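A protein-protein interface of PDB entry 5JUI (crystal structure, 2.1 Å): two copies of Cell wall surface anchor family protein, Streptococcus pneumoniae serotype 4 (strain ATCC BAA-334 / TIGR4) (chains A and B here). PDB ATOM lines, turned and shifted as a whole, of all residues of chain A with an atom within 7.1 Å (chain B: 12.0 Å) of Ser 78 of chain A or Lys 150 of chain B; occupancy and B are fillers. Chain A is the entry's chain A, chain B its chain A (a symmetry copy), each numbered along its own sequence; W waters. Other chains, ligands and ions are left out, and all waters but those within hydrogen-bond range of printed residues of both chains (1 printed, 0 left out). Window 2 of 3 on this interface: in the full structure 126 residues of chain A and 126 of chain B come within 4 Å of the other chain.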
ATOM      1  N   TYR A  41     -23.566  26.148 -14.324  1.00  0.00           N
ATOM      2  CA  TYR A  41     -22.516  26.473 -13.369  1.00  0.00           C
ATOM      3  C   TYR A  41     -21.236  26.990 -14.021  1.00  0.00           C
ATOM      4  O   TYR A  41     -20.254  27.265 -13.328  1.00  0.00           O
ATOM      5  CB  TYR A  41     -22.228  25.276 -12.461  1.00  0.00           C
ATOM      6  CG  TYR A  41     -23.397  24.959 -11.560  1.00  0.00           C
ATOM      7  CD1 TYR A  41     -23.601  25.665 -10.384  1.00  0.00           C
ATOM      8  CD2 TYR A  41     -24.299  23.960 -11.888  1.00  0.00           C
ATOM      9  CE1 TYR A  41     -24.677  25.390  -9.564  1.00  0.00           C
ATOM     10  CE2 TYR A  41     -25.375  23.674 -11.070  1.00  0.00           C
ATOM     11  CZ  TYR A  41     -25.559  24.392  -9.910  1.00  0.00           C
ATOM     12  OH  TYR A  41     -26.628  24.113  -9.092  1.00  0.00           O
ATOM     13  N   TYR A  66     -17.491  15.527 -13.994  1.00  0.00           N
ATOM     14  CA  TYR A  66     -16.912  16.859 -13.863  1.00  0.00           C
ATOM     15  C   TYR A  66     -15.430  16.776 -13.500  1.00  0.00           C
ATOM     16  O   TYR A  66     -14.779  17.794 -13.264  1.00  0.00           O
ATOM     17  CB  TYR A  66     -17.681  17.675 -12.821  1.00  0.00           C
ATOM     18  CG  TYR A  66     -19.075  18.055 -13.271  1.00  0.00           C
ATOM     19  CD1 TYR A  66     -19.311  19.239 -13.955  1.00  0.00           C
ATOM     20  CD2 TYR A  66     -20.149  17.210 -13.040  1.00  0.00           C
ATOM     21  CE1 TYR A  66     -20.592  19.582 -14.375  1.00  0.00           C
ATOM     22  CE2 TYR A  66     -21.429  17.543 -13.457  1.00  0.00           C
ATOM     23  CZ  TYR A  66     -21.643  18.726 -14.124  1.00  0.00           C
ATOM     24  OH  TYR A  66     -22.914  19.051 -14.541  1.00  0.00           O
ATOM     25  N   LEU A  74     -11.147  17.294 -10.117  1.00  0.00           N
ATOM     26  CA  LEU A  74     -12.531  17.728 -10.175  1.00  0.00           C
ATOM     27  C   LEU A  74     -12.585  19.240 -10.335  1.00  0.00           C
ATOM     28  O   LEU A  74     -11.884  19.964  -9.633  1.00  0.00           O
ATOM     29  CB  LEU A  74     -13.263  17.306  -8.900  1.00  0.00           C
ATOM     30  CG  LEU A  74     -14.707  17.773  -8.716  1.00  0.00           C
ATOM     31  CD1 LEU A  74     -15.601  17.212  -9.814  1.00  0.00           C
ATOM     32  CD2 LEU A  74     -15.230  17.382  -7.337  1.00  0.00           C
ATOM     33  N   GLY A  75     -13.412  19.721 -11.257  1.00  0.00           N
ATOM     34  CA  GLY A  75     -13.611  21.151 -11.411  1.00  0.00           C
ATOM     35  C   GLY A  75     -14.242  21.760 -10.169  1.00  0.00           C
ATOM     36  O   GLY A  75     -14.697  21.036  -9.284  1.00  0.00           O
ATOM     37  N   ASN A  76     -14.267  23.085 -10.094  1.00  0.00           N
ATOM     38  CA  ASN A  76     -14.853  23.760  -8.942  1.00  0.00           C
ATOM     39  C   ASN A  76     -16.367  23.844  -9.051  1.00  0.00           C
ATOM     40  O   ASN A  76     -16.902  24.748  -9.691  1.00  0.00           O
ATOM     41  CB  ASN A  76     -14.263  25.160  -8.765  1.00  0.00           C
ATOM     42  CG  ASN A  76     -14.841  25.893  -7.562  1.00  0.00           C
ATOM     43  OD1 ASN A  76     -15.411  25.278  -6.657  1.00  0.00           O
ATOM     44  ND2 ASN A  76     -14.696  27.213  -7.548  1.00  0.00           N
ATOM     45  N   ILE A  77     -17.048  22.890  -8.430  1.00  0.00           N
ATOM     46  CA  ILE A  77     -18.502  22.869  -8.436  1.00  0.00           C
ATOM     47  C   ILE A  77     -19.017  22.889  -7.003  1.00  0.00           C
ATOM     48  O   ILE A  77     -20.038  22.282  -6.688  1.00  0.00           O
ATOM     49  CB  ILE A  77     -19.054  21.626  -9.182  1.00  0.00           C
ATOM     50  CG1 ILE A  77     -18.409  20.340  -8.658  1.00  0.00           C
ATOM     51  CG2 ILE A  77     -18.799  21.743 -10.668  1.00  0.00           C
ATOM     52  CD1 ILE A  77     -18.971  19.074  -9.290  1.00  0.00           C
ATOM     53  N   SER A  78     -18.307  23.605  -6.135  1.00  0.00           N
ATOM     54  CA  SER A  78     -18.690  23.702  -4.730  1.00  0.00           C
ATOM     55  C   SER A  78     -20.050  24.374  -4.583  1.00  0.00           C
ATOM     56  O   SER A  78     -20.771  24.138  -3.614  1.00  0.00           O
ATOM     57  CB  SER A  78     -17.630  24.474  -3.936  1.00  0.00           C
ATOM     58  OG  SER A  78     -17.352  25.726  -4.540  1.00  0.00           O
ATOM     59  N   SER A  79     -20.403  25.200  -5.563  1.00  0.00           N
ATOM     60  CA  SER A  79     -21.672  25.915  -5.528  1.00  0.00           C
ATOM     61  C   SER A  79     -22.791  25.119  -6.197  1.00  0.00           C
ATOM     62  O   SER A  79     -23.923  25.594  -6.290  1.00  0.00           O
ATOM     63  CB  SER A  79     -21.532  27.288  -6.187  1.00  0.00           C
ATOM     64  OG  SER A  79     -21.119  27.160  -7.534  1.00  0.00           O
ATOM     65  N   MET A  80     -22.481  23.913  -6.664  1.00  0.00           N
ATOM     66  CA  MET A  80     -23.497  23.072  -7.292  1.00  0.00           C
ATOM     67  C   MET A  80     -24.437  22.561  -6.208  1.00  0.00           C
ATOM     68  O   MET A  80     -23.990  22.014  -5.197  1.00  0.00           O
ATOM     69  CB  MET A  80     -22.859  21.911  -8.064  1.00  0.00           C
ATOM     70  CG  MET A  80     -23.861  20.989  -8.756  1.00  0.00           C
ATOM     71  SD  MET A  80     -23.099  19.581  -9.603  1.00  0.00           S
ATOM     72  CE  MET A  80     -22.250  20.403 -10.954  1.00  0.00           C
ATOM     73  N   ARG A  81     -25.738  22.753  -6.399  1.00  0.00           N
ATOM     74  CA  ARG A  81     -26.683  22.333  -5.377  1.00  0.00           C
ATOM     75  C   ARG A  81     -26.848  20.824  -5.467  1.00  0.00           C
ATOM     76  O   ARG A  81     -26.719  20.242  -6.546  1.00  0.00           O
ATOM     77  CB  ARG A  81     -28.029  23.056  -5.525  1.00  0.00           C
ATOM     78  CG  ARG A  81     -28.961  22.446  -6.550  1.00  0.00           C
ATOM     79  CD  ARG A  81     -30.297  23.168  -6.586  1.00  0.00           C
ATOM     80  NE  ARG A  81     -31.224  22.524  -7.510  1.00  0.00           N
ATOM     81  CZ  ARG A  81     -31.337  22.841  -8.797  1.00  0.00           C
ATOM     82  NH1 ARG A  81     -30.577  23.797  -9.316  1.00  0.00           N
ATOM     83  NH2 ARG A  81     -32.209  22.202  -9.564  1.00  0.00           N
ATOM     84  N   PRO A  82     -27.108  20.177  -4.324  1.00  0.00           N
ATOM     85  CA  PRO A  82     -27.185  18.716  -4.276  1.00  0.00           C
ATOM     86  C   PRO A  82     -28.335  18.146  -5.092  1.00  0.00           C
ATOM     87  O   PRO A  82     -28.268  16.977  -5.476  1.00  0.00           O
ATOM     88  CB  PRO A  82     -27.406  18.431  -2.787  1.00  0.00           C
ATOM     89  CG  PRO A  82     -26.828  19.613  -2.092  1.00  0.00           C
ATOM     90  CD  PRO A  82     -27.162  20.772  -2.978  1.00  0.00           C
ATOM     91  N   GLN B 143     -29.748   9.363 -14.319  1.00  0.00           N
ATOM     92  CA  GLN B 143     -29.267  10.700 -14.001  1.00  0.00           C
ATOM     93  C   GLN B 143     -28.332  10.686 -12.805  1.00  0.00           C
ATOM     94  O   GLN B 143     -28.367   9.767 -11.985  1.00  0.00           O
ATOM     95  CB  GLN B 143     -30.443  11.649 -13.746  1.00  0.00           C
ATOM     96  CG  GLN B 143     -31.353  11.208 -12.615  1.00  0.00           C
ATOM     97  CD  GLN B 143     -32.558  12.111 -12.452  1.00  0.00           C
ATOM     98  OE1 GLN B 143     -32.538  13.058 -11.667  1.00  0.00           O
ATOM     99  NE2 GLN B 143     -33.615  11.820 -13.194  1.00  0.00           N
ATOM    100  N   MET B 144     -27.477  11.700 -12.737  1.00  0.00           N
ATOM    101  CA  MET B 144     -26.591  11.905 -11.602  1.00  0.00           C
ATOM    102  C   MET B 144     -26.876  13.247 -10.953  1.00  0.00           C
ATOM    103  O   MET B 144     -26.991  14.259 -11.648  1.00  0.00           O
ATOM    104  CB  MET B 144     -25.123  11.849 -12.029  1.00  0.00           C
ATOM    105  CG  MET B 144     -24.157  12.098 -10.872  1.00  0.00           C
ATOM    106  SD  MET B 144     -22.428  11.754 -11.256  1.00  0.00           S
ATOM    107  CE  MET B 144     -22.099  13.010 -12.488  1.00  0.00           C
ATOM    108  N   ASN B 145     -26.972  13.263  -9.628  1.00  0.00           N
ATOM    109  CA  ASN B 145     -27.247  14.507  -8.915  1.00  0.00           C
ATOM    110  C   ASN B 145     -25.976  15.231  -8.463  1.00  0.00           C
ATOM    111  O   ASN B 145     -24.875  14.675  -8.537  1.00  0.00           O
ATOM    112  CB  ASN B 145     -28.200  14.267  -7.734  1.00  0.00           C
ATOM    113  CG  ASN B 145     -27.629  13.319  -6.689  1.00  0.00           C
ATOM    114  OD1 ASN B 145     -26.427  13.308  -6.420  1.00  0.00           O
ATOM    115  ND2 ASN B 145     -28.500  12.514  -6.095  1.00  0.00           N
ATOM    116  N   GLY B 146     -26.131  16.476  -8.022  1.00  0.00           N
ATOM    117  CA  GLY B 146     -25.002  17.275  -7.577  1.00  0.00           C
ATOM    118  C   GLY B 146     -24.268  16.652  -6.402  1.00  0.00           C
ATOM    119  O   GLY B 146     -23.047  16.778  -6.291  1.00  0.00           O
ATOM    120  N   PHE B 147     -25.014  15.979  -5.530  1.00  0.00           N
ATOM    121  CA  PHE B 147     -24.445  15.292  -4.374  1.00  0.00           C
ATOM    122  C   PHE B 147     -23.373  14.293  -4.811  1.00  0.00           C
ATOM    123  O   PHE B 147     -22.306  14.218  -4.207  1.00  0.00           O
ATOM    124  CB  PHE B 147     -25.558  14.580  -3.595  1.00  0.00           C
ATOM    125  CG  PHE B 147     -25.076  13.790  -2.405  1.00  0.00           C
ATOM    126  CD1 PHE B 147     -24.642  14.430  -1.255  1.00  0.00           C
ATOM    127  CD2 PHE B 147     -25.059  12.403  -2.440  1.00  0.00           C
ATOM    128  CE1 PHE B 147     -24.200  13.695  -0.157  1.00  0.00           C
ATOM    129  CE2 PHE B 147     -24.619  11.668  -1.350  1.00  0.00           C
ATOM    130  CZ  PHE B 147     -24.190  12.314  -0.208  1.00  0.00           C
ATOM    131  N   PHE B 148     -23.655  13.542  -5.872  1.00  0.00           N
ATOM    132  CA  PHE B 148     -22.692  12.582  -6.405  1.00  0.00           C
ATOM    133  C   PHE B 148     -21.590  13.265  -7.208  1.00  0.00           C
ATOM    134  O   PHE B 148     -20.418  12.923  -7.071  1.00  0.00           O
ATOM    135  CB  PHE B 148     -23.388  11.532  -7.277  1.00  0.00           C
ATOM    136  CG  PHE B 148     -24.155  10.500  -6.496  1.00  0.00           C
ATOM    137  CD1 PHE B 148     -23.683  10.034  -5.276  1.00  0.00           C
ATOM    138  CD2 PHE B 148     -25.330   9.966  -7.001  1.00  0.00           C
ATOM    139  CE1 PHE B 148     -24.382   9.071  -4.564  1.00  0.00           C
ATOM    140  CE2 PHE B 148     -26.033   9.001  -6.294  1.00  0.00           C
ATOM    141  CZ  PHE B 148     -25.560   8.554  -5.074  1.00  0.00           C
ATOM    142  N   ALA B 149     -21.979  14.199  -8.072  1.00  0.00           N
ATOM    143  CA  ALA B 149     -21.033  14.935  -8.909  1.00  0.00           C
ATOM    144  C   ALA B 149     -19.908  15.557  -8.093  1.00  0.00           C
ATOM    145  O   ALA B 149     -18.736  15.492  -8.471  1.00  0.00           O
ATOM    146  CB  ALA B 149     -21.761  16.006  -9.708  1.00  0.00           C
ATOM    147  N   LYS B 150     -20.277  16.165  -6.972  1.00  0.00           N
ATOM    148  CA  LYS B 150     -19.321  16.854  -6.114  1.00  0.00           C
ATOM    149  C   LYS B 150     -18.375  15.899  -5.386  1.00  0.00           C
ATOM    150  O   LYS B 150     -17.367  16.328  -4.826  1.00  0.00           O
ATOM    151  CB  LYS B 150     -20.063  17.758  -5.127  1.00  0.00           C
ATOM    152  CG  LYS B 150     -20.639  19.009  -5.785  1.00  0.00           C
ATOM    153  CD  LYS B 150     -21.871  19.521  -5.056  1.00  0.00           C
ATOM    154  CE  LYS B 150     -21.500  20.255  -3.785  1.00  0.00           C
ATOM    155  NZ  LYS B 150     -22.714  20.689  -3.059  1.00  0.00           N
ATOM    156  N   LYS B 151     -18.695  14.607  -5.410  1.00  0.00           N
ATOM    157  CA  LYS B 151     -17.811  13.578  -4.870  1.00  0.00           C
ATOM    158  C   LYS B 151     -16.808  13.139  -5.933  1.00  0.00           C
ATOM    159  O   LYS B 151     -15.948  12.297  -5.683  1.00  0.00           O
ATOM    160  CB  LYS B 151     -18.609  12.363  -4.386  1.00  0.00           C
ATOM    161  CG  LYS B 151     -19.453  12.591  -3.130  1.00  0.00           C
ATOM    162  CD  LYS B 151     -20.203  11.320  -2.745  1.00  0.00           C
ATOM    163  CE  LYS B 151     -21.014  11.506  -1.473  1.00  0.00           C
ATOM    164  NZ  LYS B 151     -20.150  11.687  -0.278  1.00  0.00           N
ATOM    165  N   GLY B 152     -16.937  13.702  -7.129  1.00  0.00           N
ATOM    166  CA  GLY B 152     -16.089  13.303  -8.233  1.00  0.00           C
ATOM    167  C   GLY B 152     -16.616  12.055  -8.917  1.00  0.00           C
ATOM    168  O   GLY B 152     -15.878  11.365  -9.615  1.00  0.00           O
ATOM    169  N   TYR B 153     -17.893  11.752  -8.704  1.00  0.00           N
ATOM    170  CA  TYR B 153     -18.500  10.571  -9.317  1.00  0.00           C
ATOM    171  C   TYR B 153     -18.865  10.851 -10.767  1.00  0.00           C
ATOM    172  O   TYR B 153     -18.890  12.004 -11.201  1.00  0.00           O
ATOM    173  CB  TYR B 153     -19.757  10.140  -8.557  1.00  0.00           C
ATOM    174  CG  TYR B 153     -19.514   9.540  -7.188  1.00  0.00           C
ATOM    175  CD1 TYR B 153     -18.230   9.370  -6.690  1.00  0.00           C
ATOM    176  CD2 TYR B 153     -20.579   9.147  -6.391  1.00  0.00           C
ATOM    177  CE1 TYR B 153     -18.015   8.823  -5.435  1.00  0.00           C
ATOM    178  CE2 TYR B 153     -20.373   8.599  -5.135  1.00  0.00           C
ATOM    179  CZ  TYR B 153     -19.089   8.438  -4.665  1.00  0.00           C
ATOM    180  OH  TYR B 153     -18.883   7.894  -3.420  1.00  0.00           O
ATOM    181  N   GLY B 154     -19.167   9.790 -11.510  1.00  0.00           N
ATOM    182  CA  GLY B 154     -19.547   9.932 -12.900  1.00  0.00           C
ATOM    183  C   GLY B 154     -20.799   9.143 -13.218  1.00  0.00           C
ATOM    184  O   GLY B 154     -21.129   8.176 -12.533  1.00  0.00           O
ATOM    185  N   LEU B 155     -21.512   9.580 -14.248  1.00  0.00           N
ATOM    186  CA  LEU B 155     -22.692   8.873 -14.717  1.00  0.00           C
ATOM    187  C   LEU B 155     -22.261   8.003 -15.881  1.00  0.00           C
ATOM    188  O   LEU B 155     -21.773   8.505 -16.893  1.00  0.00           O
ATOM    189  CB  LEU B 155     -23.778   9.865 -15.148  1.00  0.00           C
ATOM    190  CG  LEU B 155     -25.112   9.320 -15.670  1.00  0.00           C
ATOM    191  CD1 LEU B 155     -25.761   8.367 -14.676  1.00  0.00           C
ATOM    192  CD2 LEU B 155     -26.049  10.481 -15.978  1.00  0.00           C
HETATM  193  O   HOH W   1     -18.059  14.513 -11.156  1.00  0.00           O
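O of Met 80 of chain A lies within hydrogen-bond range of NZ of Lys 150 of chain B (2.8 Å). The backbone carbonyl oxygen (O) of Pro 82 of chain A sits at hydrogen-bond distance from the backbone NH (N) of Gly 146 of chain B (3.4 Å). The backbone carbonyl oxygen of Pro 82 of chain A sits at hydrogen-bond distance from the backbone NH of Phe 147 of chain B.
The backbone NH (N) of Arg 81 of chain A sits at hydrogen-bond distance from the side-chain hydroxyl (OH) of Tyr 41 of chain A (3.1 Å). The backbone carbonyl oxygen (O) of Tyr 66 of chain A sits at hydrogen-bond distance from the backbone NH (N) of Gly 75 of chain A (3.1 Å). The side-chain amide oxygen of Asn 76 of chain A lies within hydrogen-bond range of the side-chain hydroxyl of Ser 78 of chain A, 2.9 Å away. OD1 of Asn 145 of chain B lies within hydrogen-bond range of N of Phe 147 of chain B (3.2 Å). OD1 of Asn 145 of chain B lies within hydrogen-bond range of N of Phe 148 of chain B (2.8 Å).
CB of Ala 149 of chain B touches CD2 of Tyr 66 of chain A, at 3.9 Å. Leu 74 of chain A touches Ala 149 of chain B (CD1 to O, 3.8 Å). Lys 150 of chain B touches Leu 74 of chain A. Ala 149 of chain B touches Ile 77 of chain A. O of Ile 77 of chain A touches CG of Lys 150 of chain B (3.4 Å). Lys 150 of chain B touches Ser 78 of chain A (CE to O, 3.95 Å). SD of Met 80 of chain A touches CA of Gly 146 of chain B, at 3.6 Å. Met 80 of chain A touches Ala 149 of chain B (SD to CB, 3.8 Å). Arg 81 of chain A touches Gly 146 of chain B (O to CA, 3.6 Å). Pro 82 of chain A touches Asn 145 of chain B.
Tyr 41 of chain A touches none of the printed residues of chain B. No residue of chain B comes within 4 Å of Asn 76 of chain A. Of chain B, only Ala 149 (3.7 Å) and Lys 150 (3.4 Å) come within 4 Å of Ile 77 of chain A. Of chain B, only Lys 150 comes within 4 Å of Ser 78 of chain A. Of chain B, only Asn 145, Gly 146 and Phe 147 come within 4 Å of Pro 82 of chain A. Printed residues of chain A within 4 Å of Phe 147 of chain B: Pro 82 (3.4 Å). Of the printed residues of chain A, Ala 149 of chain B touches Tyr 66, Leu 74, Ile 77 and Met 80. Of the printed residues of chain A, Lys 150 of chain B touches Leu 74, Ile 77, Ser 78 and Met 80. The nearest residue of chain B that does not touch Ser 78 of chain A is Gly 146 of chain B (8.2 Å).
Hydrophobic or aromatic side chains of chain B that line the printed part of chain A: Ala 149.
No position is printed for both chains. Of the 13 pairs that touch across the chains among the printed residues, none has its exchanged pair printed and touching as well.
Water W1 lies within hydrogen-bond range of O of Tyr 153 of chain B, O of Ala 149 of chain B and N of Tyr 66 of chain A.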
